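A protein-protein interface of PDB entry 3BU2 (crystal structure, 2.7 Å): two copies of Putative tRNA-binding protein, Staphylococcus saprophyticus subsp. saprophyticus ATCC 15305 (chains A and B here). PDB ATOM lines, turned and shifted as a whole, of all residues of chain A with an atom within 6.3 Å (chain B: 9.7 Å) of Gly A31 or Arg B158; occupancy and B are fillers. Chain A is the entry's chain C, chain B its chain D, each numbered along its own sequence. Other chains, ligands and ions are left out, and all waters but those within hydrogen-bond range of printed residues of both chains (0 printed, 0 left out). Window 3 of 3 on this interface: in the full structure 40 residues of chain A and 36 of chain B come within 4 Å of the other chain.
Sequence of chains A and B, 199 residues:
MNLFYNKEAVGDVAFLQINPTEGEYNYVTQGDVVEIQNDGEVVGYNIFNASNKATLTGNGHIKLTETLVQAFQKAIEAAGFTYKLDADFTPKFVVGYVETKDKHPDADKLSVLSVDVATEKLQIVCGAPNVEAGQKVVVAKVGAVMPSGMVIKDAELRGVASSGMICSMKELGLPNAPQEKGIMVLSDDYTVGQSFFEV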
ATOM      1  N   THR A  29     -18.882   0.741   9.272  1.00  0.00           N
ATOM      2  CA  THR A  29     -19.201   0.991   7.879  1.00  0.00           C
ATOM      3  C   THR A  29     -18.147   0.504   6.883  1.00  0.00           C
ATOM      4  O   THR A  29     -16.939   0.663   7.087  1.00  0.00           O
ATOM      5  CB  THR A  29     -19.475   2.492   7.641  1.00  0.00           C
ATOM      6  OG1 THR A  29     -19.479   2.756   6.230  1.00  0.00           O
ATOM      7  CG2 THR A  29     -18.423   3.351   8.333  1.00  0.00           C
ATOM      8  N   GLN A  30     -18.630  -0.110   5.806  1.00  0.00           N
ATOM      9  CA  GLN A  30     -17.789  -0.646   4.750  1.00  0.00           C
ATOM     10  C   GLN A  30     -18.587  -0.606   3.469  1.00  0.00           C
ATOM     11  O   GLN A  30     -19.564  -1.340   3.307  1.00  0.00           O
ATOM     12  CB  GLN A  30     -17.394  -2.090   5.056  1.00  0.00           C
ATOM     13  CG  GLN A  30     -16.355  -2.210   6.150  1.00  0.00           C
ATOM     14  CD  GLN A  30     -16.167  -3.640   6.651  1.00  0.00           C
ATOM     15  OE1 GLN A  30     -16.131  -4.591   5.861  1.00  0.00           O
ATOM     16  NE2 GLN A  30     -16.018  -3.791   7.972  1.00  0.00           N
ATOM     17  N   GLY A  31     -18.170   0.264   2.559  1.00  0.00           N
ATOM     18  CA  GLY A  31     -18.863   0.378   1.294  1.00  0.00           C
ATOM     19  C   GLY A  31     -20.272   0.892   1.483  1.00  0.00           C
ATOM     20  O   GLY A  31     -20.480   1.931   2.113  1.00  0.00           O
ATOM     21  N   ASP A  32     -21.243   0.164   0.940  1.00  0.00           N
ATOM     22  CA  ASP A  32     -22.634   0.558   1.058  1.00  0.00           C
ATOM     23  C   ASP A  32     -23.350  -0.080   2.232  1.00  0.00           C
ATOM     24  O   ASP A  32     -24.507   0.236   2.488  1.00  0.00           O
ATOM     25  CB  ASP A  32     -23.398   0.229  -0.222  1.00  0.00           C
ATOM     26  CG  ASP A  32     -23.179   1.258  -1.304  1.00  0.00           C
ATOM     27  OD1 ASP A  32     -22.627   2.333  -0.992  1.00  0.00           O
ATOM     28  OD2 ASP A  32     -23.569   1.001  -2.461  1.00  0.00           O
ATOM     29  N   VAL A  33     -22.695  -0.979   2.954  1.00  0.00           N
ATOM     30  CA  VAL A  33     -23.388  -1.582   4.075  1.00  0.00           C
ATOM     31  C   VAL A  33     -22.752  -1.188   5.392  1.00  0.00           C
ATOM     32  O   VAL A  33     -21.531  -1.187   5.531  1.00  0.00           O
ATOM     33  CB  VAL A  33     -23.474  -3.144   3.951  1.00  0.00           C
ATOM     34  CG1 VAL A  33     -23.034  -3.595   2.576  1.00  0.00           C
ATOM     35  CG2 VAL A  33     -22.680  -3.811   5.043  1.00  0.00           C
ATOM     36  N   VAL A  34     -23.599  -0.825   6.348  1.00  0.00           N
ATOM     37  CA  VAL A  34     -23.146  -0.436   7.667  1.00  0.00           C
ATOM     38  C   VAL A  34     -23.652  -1.500   8.615  1.00  0.00           C
ATOM     39  O   VAL A  34     -24.854  -1.750   8.686  1.00  0.00           O
ATOM     40  CB  VAL A  34     -23.729   0.930   8.094  1.00  0.00           C
ATOM     41  CG1 VAL A  34     -23.383   1.221   9.540  1.00  0.00           C
ATOM     42  CG2 VAL A  34     -23.182   2.033   7.197  1.00  0.00           C
ATOM     43  N   ASN A  46     -27.749  -1.445   7.696  1.00  0.00           N
ATOM     44  CA  ASN A  46     -28.289  -0.354   6.906  1.00  0.00           C
ATOM     45  C   ASN A  46     -27.529  -0.496   5.604  1.00  0.00           C
ATOM     46  O   ASN A  46     -26.357  -0.127   5.529  1.00  0.00           O
ATOM     47  CB  ASN A  46     -27.960   1.005   7.520  1.00  0.00           C
ATOM     48  CG  ASN A  46     -28.761   1.293   8.763  1.00  0.00           C
ATOM     49  OD1 ASN A  46     -28.570   2.320   9.396  1.00  0.00           O
ATOM     50  ND2 ASN A  46     -29.662   0.391   9.121  1.00  0.00           N
ATOM     51  N   PHE A  48     -27.120   0.721   1.910  1.00  0.00           N
ATOM     52  CA  PHE A  48     -27.482   1.835   1.048  1.00  0.00           C
ATOM     53  C   PHE A  48     -27.481   1.461  -0.421  1.00  0.00           C
ATOM     54  O   PHE A  48     -26.774   0.544  -0.831  1.00  0.00           O
ATOM     55  CB  PHE A  48     -26.542   3.008   1.321  1.00  0.00           C
ATOM     56  CG  PHE A  48     -26.492   3.399   2.778  1.00  0.00           C
ATOM     57  CD1 PHE A  48     -25.754   2.638   3.695  1.00  0.00           C
ATOM     58  CD2 PHE A  48     -27.256   4.474   3.255  1.00  0.00           C
ATOM     59  CE1 PHE A  48     -25.774   2.941   5.071  1.00  0.00           C
ATOM     60  CE2 PHE A  48     -27.286   4.787   4.629  1.00  0.00           C
ATOM     61  CZ  PHE A  48     -26.545   4.014   5.540  1.00  0.00           C
ATOM     62  N   ALA A  79     -19.232  -6.623   0.963  1.00  0.00           N
ATOM     63  CA  ALA A  79     -18.725  -5.462   1.691  1.00  0.00           C
ATOM     64  C   ALA A  79     -17.618  -5.892   2.642  1.00  0.00           C
ATOM     65  O   ALA A  79     -16.933  -5.050   3.227  1.00  0.00           O
ATOM     66  CB  ALA A  79     -19.854  -4.784   2.468  1.00  0.00           C
ATOM     67  N   PHE A  81     -18.089  -8.123   5.374  1.00  0.00           N
ATOM     68  CA  PHE A  81     -18.573  -8.651   6.640  1.00  0.00           C
ATOM     69  C   PHE A  81     -18.728 -10.157   6.552  1.00  0.00           C
ATOM     70  O   PHE A  81     -19.016 -10.686   5.485  1.00  0.00           O
ATOM     71  CB  PHE A  81     -19.898  -7.982   6.984  1.00  0.00           C
ATOM     72  CG  PHE A  81     -19.770  -6.507   7.226  1.00  0.00           C
ATOM     73  CD1 PHE A  81     -19.288  -6.027   8.442  1.00  0.00           C
ATOM     74  CD2 PHE A  81     -20.073  -5.596   6.222  1.00  0.00           C
ATOM     75  CE1 PHE A  81     -19.103  -4.672   8.649  1.00  0.00           C
ATOM     76  CE2 PHE A  81     -19.891  -4.232   6.422  1.00  0.00           C
ATOM     77  CZ  PHE A  81     -19.405  -3.771   7.637  1.00  0.00           C
ATOM     78  N   ASP B  12     -33.075   5.494  -0.528  1.00  0.00           N
ATOM     79  CA  ASP B  12     -32.787   4.178  -1.075  1.00  0.00           C
ATOM     80  C   ASP B  12     -31.938   3.449  -0.045  1.00  0.00           C
ATOM     81  O   ASP B  12     -30.760   3.188  -0.275  1.00  0.00           O
ATOM     82  CB  ASP B  12     -32.023   4.290  -2.396  1.00  0.00           C
ATOM     83  CG  ASP B  12     -32.066   3.005  -3.200  1.00  0.00           C
ATOM     84  OD1 ASP B  12     -31.360   2.925  -4.223  1.00  0.00           O
ATOM     85  OD2 ASP B  12     -32.808   2.072  -2.822  1.00  0.00           O
ATOM     86  N   VAL B  13     -32.545   3.141   1.098  1.00  0.00           N
ATOM     87  CA  VAL B  13     -31.850   2.447   2.168  1.00  0.00           C
ATOM     88  C   VAL B  13     -32.700   1.353   2.787  1.00  0.00           C
ATOM     89  O   VAL B  13     -33.767   1.614   3.352  1.00  0.00           O
ATOM     90  CB  VAL B  13     -31.423   3.403   3.307  1.00  0.00           C
ATOM     91  CG1 VAL B  13     -30.717   2.624   4.400  1.00  0.00           C
ATOM     92  CG2 VAL B  13     -30.493   4.469   2.775  1.00  0.00           C
ATOM     93  N   PHE B  15     -33.454  -1.180   5.580  1.00  0.00           N
ATOM     94  CA  PHE B  15     -33.235  -1.287   7.013  1.00  0.00           C
ATOM     95  C   PHE B  15     -33.432  -2.703   7.541  1.00  0.00           C
ATOM     96  O   PHE B  15     -34.559  -3.212   7.575  1.00  0.00           O
ATOM     97  CB  PHE B  15     -34.190  -0.358   7.750  1.00  0.00           C
ATOM     98  CG  PHE B  15     -33.822   1.089   7.657  1.00  0.00           C
ATOM     99  CD1 PHE B  15     -32.722   1.583   8.345  1.00  0.00           C
ATOM    100  CD2 PHE B  15     -34.593   1.967   6.899  1.00  0.00           C
ATOM    101  CE1 PHE B  15     -32.397   2.932   8.282  1.00  0.00           C
ATOM    102  CE2 PHE B  15     -34.277   3.319   6.830  1.00  0.00           C
ATOM    103  CZ  PHE B  15     -33.179   3.803   7.521  1.00  0.00           C
ATOM    104  N   LYS B 103     -27.298  19.567   2.889  1.00  0.00           N
ATOM    105  CA  LYS B 103     -26.893  18.390   2.146  1.00  0.00           C
ATOM    106  C   LYS B 103     -26.116  17.455   3.055  1.00  0.00           C
ATOM    107  O   LYS B 103     -25.347  17.901   3.902  1.00  0.00           O
ATOM    108  CB  LYS B 103     -26.021  18.792   0.954  1.00  0.00           C
ATOM    109  CG  LYS B 103     -26.795  19.228  -0.275  1.00  0.00           C
ATOM    110  CD  LYS B 103     -27.605  18.072  -0.883  1.00  0.00           C
ATOM    111  CE  LYS B 103     -26.717  17.040  -1.590  1.00  0.00           C
ATOM    112  NZ  LYS B 103     -25.825  16.284  -0.656  1.00  0.00           N
ATOM    113  N   HIS B 104     -26.336  16.155   2.890  1.00  0.00           N
ATOM    114  CA  HIS B 104     -25.619  15.169   3.684  1.00  0.00           C
ATOM    115  C   HIS B 104     -24.193  15.218   3.147  1.00  0.00           C
ATOM    116  O   HIS B 104     -23.972  15.113   1.938  1.00  0.00           O
ATOM    117  CB  HIS B 104     -26.233  13.782   3.480  1.00  0.00           C
ATOM    118  CG  HIS B 104     -25.636  12.721   4.348  1.00  0.00           C
ATOM    119  ND1 HIS B 104     -24.291  12.420   4.339  1.00  0.00           N
ATOM    120  CD2 HIS B 104     -26.209  11.854   5.217  1.00  0.00           C
ATOM    121  CE1 HIS B 104     -24.063  11.412   5.160  1.00  0.00           C
ATOM    122  NE2 HIS B 104     -25.211  11.050   5.705  1.00  0.00           N
ATOM    123  N   PRO B 105     -23.203  15.382   4.035  1.00  0.00           N
ATOM    124  CA  PRO B 105     -21.802  15.451   3.607  1.00  0.00           C
ATOM    125  C   PRO B 105     -21.374  14.418   2.564  1.00  0.00           C
ATOM    126  O   PRO B 105     -20.629  14.745   1.644  1.00  0.00           O
ATOM    127  CB  PRO B 105     -21.028  15.349   4.927  1.00  0.00           C
ATOM    128  CG  PRO B 105     -21.958  14.601   5.824  1.00  0.00           C
ATOM    129  CD  PRO B 105     -23.292  15.224   5.495  1.00  0.00           C
ATOM    130  N   ASP B 106     -21.853  13.187   2.692  1.00  0.00           N
ATOM    131  CA  ASP B 106     -21.505  12.154   1.723  1.00  0.00           C
ATOM    132  C   ASP B 106     -22.596  11.099   1.516  1.00  0.00           C
ATOM    133  O   ASP B 106     -22.417   9.925   1.846  1.00  0.00           O
ATOM    134  CB  ASP B 106     -20.183  11.481   2.118  1.00  0.00           C
ATOM    135  CG  ASP B 106     -20.182  11.007   3.555  1.00  0.00           C
ATOM    136  OD1 ASP B 106     -21.009  10.134   3.880  1.00  0.00           O
ATOM    137  OD2 ASP B 106     -19.361  11.516   4.357  1.00  0.00           O
ATOM    138  N   ALA B 107     -23.727  11.533   0.964  1.00  0.00           N
ATOM    139  CA  ALA B 107     -24.852  10.649   0.666  1.00  0.00           C
ATOM    140  C   ALA B 107     -25.467  11.089  -0.659  1.00  0.00           C
ATOM    141  O   ALA B 107     -25.950  10.261  -1.440  1.00  0.00           O
ATOM    142  CB  ALA B 107     -25.892  10.700   1.783  1.00  0.00           C
ATOM    143  N   ASP B 108     -25.449  12.399  -0.892  1.00  0.00           N
ATOM    144  CA  ASP B 108     -25.948  13.006  -2.128  1.00  0.00           C
ATOM    145  C   ASP B 108     -27.455  13.180  -2.293  1.00  0.00           C
ATOM    146  O   ASP B 108     -27.915  14.260  -2.651  1.00  0.00           O
ATOM    147  CB  ASP B 108     -25.396  12.250  -3.340  1.00  0.00           C
ATOM    148  CG  ASP B 108     -25.847  12.854  -4.650  1.00  0.00           C
ATOM    149  OD1 ASP B 108     -25.670  14.079  -4.824  1.00  0.00           O
ATOM    150  OD2 ASP B 108     -26.378  12.108  -5.504  1.00  0.00           O
ATOM    151  N   LYS B 109     -28.226  12.124  -2.060  1.00  0.00           N
ATOM    152  CA  LYS B 109     -29.675  12.227  -2.192  1.00  0.00           C
ATOM    153  C   LYS B 109     -30.366  12.281  -0.832  1.00  0.00           C
ATOM    154  O   LYS B 109     -31.577  12.082  -0.727  1.00  0.00           O
ATOM    155  CB  LYS B 109     -30.224  11.055  -3.003  1.00  0.00           C
ATOM    156  CG  LYS B 109     -29.947  11.159  -4.493  1.00  0.00           C
ATOM    157  CD  LYS B 109     -30.451   9.929  -5.224  1.00  0.00           C
ATOM    158  CE  LYS B 109     -29.708   8.680  -4.754  1.00  0.00           C
ATOM    159  NZ  LYS B 109     -30.269   7.444  -5.350  1.00  0.00           N
ATOM    160  N   LEU B 110     -29.583  12.547   0.205  1.00  0.00           N
ATOM    161  CA  LEU B 110     -30.108  12.650   1.554  1.00  0.00           C
ATOM    162  C   LEU B 110     -29.777  14.021   2.114  1.00  0.00           C
ATOM    163  O   LEU B 110     -28.774  14.630   1.750  1.00  0.00           O
ATOM    164  CB  LEU B 110     -29.492  11.587   2.471  1.00  0.00           C
ATOM    165  CG  LEU B 110     -29.662  10.092   2.182  1.00  0.00           C
ATOM    166  CD1 LEU B 110     -28.955   9.302   3.284  1.00  0.00           C
ATOM    167  CD2 LEU B 110     -31.135   9.710   2.125  1.00  0.00           C
ATOM    168  N   VAL B 112     -29.721  16.387   5.903  1.00  0.00           N
ATOM    169  CA  VAL B 112     -29.723  16.258   7.340  1.00  0.00           C
ATOM    170  C   VAL B 112     -30.552  17.462   7.762  1.00  0.00           C
ATOM    171  O   VAL B 112     -30.308  18.586   7.318  1.00  0.00           O
ATOM    172  CB  VAL B 112     -28.288  16.303   7.944  1.00  0.00           C
ATOM    173  CG1 VAL B 112     -27.260  15.939   6.875  1.00  0.00           C
ATOM    174  CG2 VAL B 112     -28.003  17.653   8.550  1.00  0.00           C
ATOM    175  N   GLN B 123     -31.896  16.016  15.324  1.00  0.00           N
ATOM    176  CA  GLN B 123     -31.185  16.009  14.062  1.00  0.00           C
ATOM    177  C   GLN B 123     -31.572  14.697  13.398  1.00  0.00           C
ATOM    178  O   GLN B 123     -31.192  13.632  13.864  1.00  0.00           O
ATOM    179  CB  GLN B 123     -29.675  16.058  14.273  1.00  0.00           C
ATOM    180  CG  GLN B 123     -28.910  15.761  12.992  1.00  0.00           C
ATOM    181  CD  GLN B 123     -27.419  15.886  13.145  1.00  0.00           C
ATOM    182  OE1 GLN B 123     -26.906  16.977  13.317  1.00  0.00           O
ATOM    183  NE2 GLN B 123     -26.715  14.762  13.082  1.00  0.00           N
ATOM    184  N   VAL B 125     -31.922  12.508   9.623  1.00  0.00           N
ATOM    185  CA  VAL B 125     -31.502  12.476   8.232  1.00  0.00           C
ATOM    186  C   VAL B 125     -32.673  11.996   7.404  1.00  0.00           C
ATOM    187  O   VAL B 125     -33.266  10.961   7.699  1.00  0.00           O
ATOM    188  CB  VAL B 125     -30.315  11.533   8.032  1.00  0.00           C
ATOM    189  CG1 VAL B 125     -30.022  11.376   6.562  1.00  0.00           C
ATOM    190  CG2 VAL B 125     -29.091  12.095   8.751  1.00  0.00           C
ATOM    191  N   ALA B 155     -30.530   6.012  15.531  1.00  0.00           N
ATOM    192  CA  ALA B 155     -29.774   5.557  14.380  1.00  0.00           C
ATOM    193  C   ALA B 155     -28.630   6.460  13.947  1.00  0.00           C
ATOM    194  O   ALA B 155     -28.198   7.353  14.675  1.00  0.00           O
ATOM    195  CB  ALA B 155     -30.726   5.333  13.204  1.00  0.00           C
ATOM    196  N   GLU B 156     -28.163   6.191  12.731  1.00  0.00           N
ATOM    197  CA  GLU B 156     -27.068   6.901  12.097  1.00  0.00           C
ATOM    198  C   GLU B 156     -27.103   6.502  10.619  1.00  0.00           C
ATOM    199  O   GLU B 156     -27.079   5.316  10.291  1.00  0.00           O
ATOM    200  CB  GLU B 156     -25.746   6.466  12.734  1.00  0.00           C
ATOM    201  CG  GLU B 156     -24.513   7.036  12.072  1.00  0.00           C
ATOM    202  CD  GLU B 156     -23.231   6.573  12.735  1.00  0.00           C
ATOM    203  OE1 GLU B 156     -23.027   6.875  13.927  1.00  0.00           O
ATOM    204  OE2 GLU B 156     -22.428   5.904  12.056  1.00  0.00           O
ATOM    205  N   LEU B 157     -27.189   7.487   9.733  1.00  0.00           N
ATOM    206  CA  LEU B 157     -27.224   7.211   8.298  1.00  0.00           C
ATOM    207  C   LEU B 157     -25.966   7.706   7.592  1.00  0.00           C
ATOM    208  O   LEU B 157     -25.755   8.911   7.440  1.00  0.00           O
ATOM    209  CB  LEU B 157     -28.448   7.856   7.652  1.00  0.00           C
ATOM    210  CG  LEU B 157     -29.521   6.885   7.167  1.00  0.00           C
ATOM    211  CD1 LEU B 157     -30.086   6.138   8.364  1.00  0.00           C
ATOM    212  CD2 LEU B 157     -30.626   7.640   6.438  1.00  0.00           C
ATOM    213  N   ARG B 158     -25.144   6.761   7.155  1.00  0.00           N
ATOM    214  CA  ARG B 158     -23.898   7.065   6.470  1.00  0.00           C
ATOM    215  C   ARG B 158     -23.075   8.124   7.172  1.00  0.00           C
ATOM    216  O   ARG B 158     -22.701   9.124   6.566  1.00  0.00           O
ATOM    217  CB  ARG B 158     -24.153   7.500   5.024  1.00  0.00           C
ATOM    218  CG  ARG B 158     -24.718   6.392   4.152  1.00  0.00           C
ATOM    219  CD  ARG B 158     -24.454   6.620   2.676  1.00  0.00           C
ATOM    220  NE  ARG B 158     -23.072   6.325   2.315  1.00  0.00           N
ATOM    221  CZ  ARG B 158     -22.521   5.118   2.389  1.00  0.00           C
ATOM    222  NH1 ARG B 158     -21.252   4.940   2.040  1.00  0.00           N
ATOM    223  NH2 ARG B 158     -23.238   4.083   2.810  1.00  0.00           N
ATOM    224  N   GLY B 159     -22.809   7.916   8.456  1.00  0.00           N
ATOM    225  CA  GLY B 159     -21.986   8.865   9.177  1.00  0.00           C
ATOM    226  C   GLY B 159     -22.657   9.769  10.181  1.00  0.00           C
ATOM    227  O   GLY B 159     -22.280   9.781  11.356  1.00  0.00           O
ATOM    228  N   VAL B 160     -23.641  10.539   9.732  1.00  0.00           N
ATOM    229  CA  VAL B 160     -24.328  11.465  10.629  1.00  0.00           C
ATOM    230  C   VAL B 160     -25.480  10.824  11.397  1.00  0.00           C
ATOM    231  O   VAL B 160     -26.244  10.037  10.840  1.00  0.00           O
ATOM    232  CB  VAL B 160     -24.829  12.716   9.851  1.00  0.00           C
ATOM    233  CG1 VAL B 160     -24.690  12.491   8.359  1.00  0.00           C
ATOM    234  CG2 VAL B 160     -26.270  13.037  10.234  1.00  0.00           C
ATOM    235  N   ALA B 161     -25.589  11.175  12.678  1.00  0.00           N
ATOM    236  CA  ALA B 161     -26.630  10.636  13.551  1.00  0.00           C
ATOM    237  C   ALA B 161     -28.023  11.095  13.146  1.00  0.00           C
ATOM    238  O   ALA B 161     -28.198  12.197  12.621  1.00  0.00           O
ATOM    239  CB  ALA B 161     -26.357  11.031  14.997  1.00  0.00           C
ATOM    240  N   SER B 162     -29.008  10.239  13.404  1.00  0.00           N
ATOM    241  CA  SER B 162     -30.402  10.517  13.069  1.00  0.00           C
ATOM    242  C   SER B 162     -31.312  10.039  14.198  1.00  0.00           C
ATOM    243  O   SER B 162     -31.432   8.842  14.443  1.00  0.00           O
ATOM    244  CB  SER B 162     -30.768   9.801  11.762  1.00  0.00           C
ATOM    245  OG  SER B 162     -32.105  10.059  11.381  1.00  0.00           O
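The side-chain amide oxygen (OD1) of Asn A46 lies close to the backbone carbonyl oxygen (O) of Glu B156 (3.5 Å).
NH1 of Arg B158 is in hydrogen-bond range of O of Gly A31 (3.1 Å).
Arg B158 touches Asp A32 (NH2 to CA, 3.98 Å).
Phe B15 touches Asn A46.
Phe A48 touches Asp B12 (C to O, 3.7 Å).
CG2 of Val B13 touches CD2 of Phe A48, 3.3 Å away.
Phe A48 touches Leu B157 (CE2 to CG, 3.98 Å).
NH2 of Arg B158 touches CD1 of Phe A48, 3.0 Å away.
The backbone carbonyl oxygen (O) of Asn A46 is in hydrogen-bond range of the backbone NH (N) of Val A34 (3.0 Å).
O of Arg B158 lies close to NE2 of His B104 (3.3 Å).
N of Phe A48 lies within hydrogen-bond range of O of Asp A32 (2.7 Å).
A ring nitrogen (NE2) of His B104 is in hydrogen-bond range of the backbone carbonyl oxygen (O) of Leu B157 (2.8 Å).
Of the 22 printed residues of chain B, 6 touch a printed residue of chain A.
Hydrophobic or aromatic side chains of chain B that line the printed part of chain A: Val B13, Phe B15 and Leu B157.
Hydrophobic or aromatic side chains of chain A within 4 Å of the printed part of chain B: Phe A48.
Among the printed residues, no Asp or Glu carboxylate lies within 4 Å of a Lys or Arg side-chain nitrogen of the other chain.
Gly A31 touches just one residue of chain B: Arg B158 (3.1 Å).
Printed residues of chain B within 4 Å of Asp A32: Arg B158.
Val A34 touches none of the printed residues of chain B.
Printed residues of chain B within 4 Å of Asn A46: Phe B15 (3.4 Å) and Glu B156 (3.5 Å).
Printed residues of chain B within 4 Å of Phe A48: Asp B12 (3.7 Å), Val B13 (3.3 Å), Leu B157 (3.98 Å) and Arg B158 (3.0 Å).
Printed residues of chain A within 4 Å of Asp B12: Phe A48.
Ala B155 touches none of the printed residues of chain A.
Printed residues of chain A within 4 Å of Glu B156: Asn A46 (3.5 Å).
Of the printed residues of chain A, Arg B158 touches Gly A31, Asp A32 and Phe A48.
The nearest printed residue of chain A that does not touch Asp B12 is Asp A32 (7.4 Å).
No position is printed for both chains.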
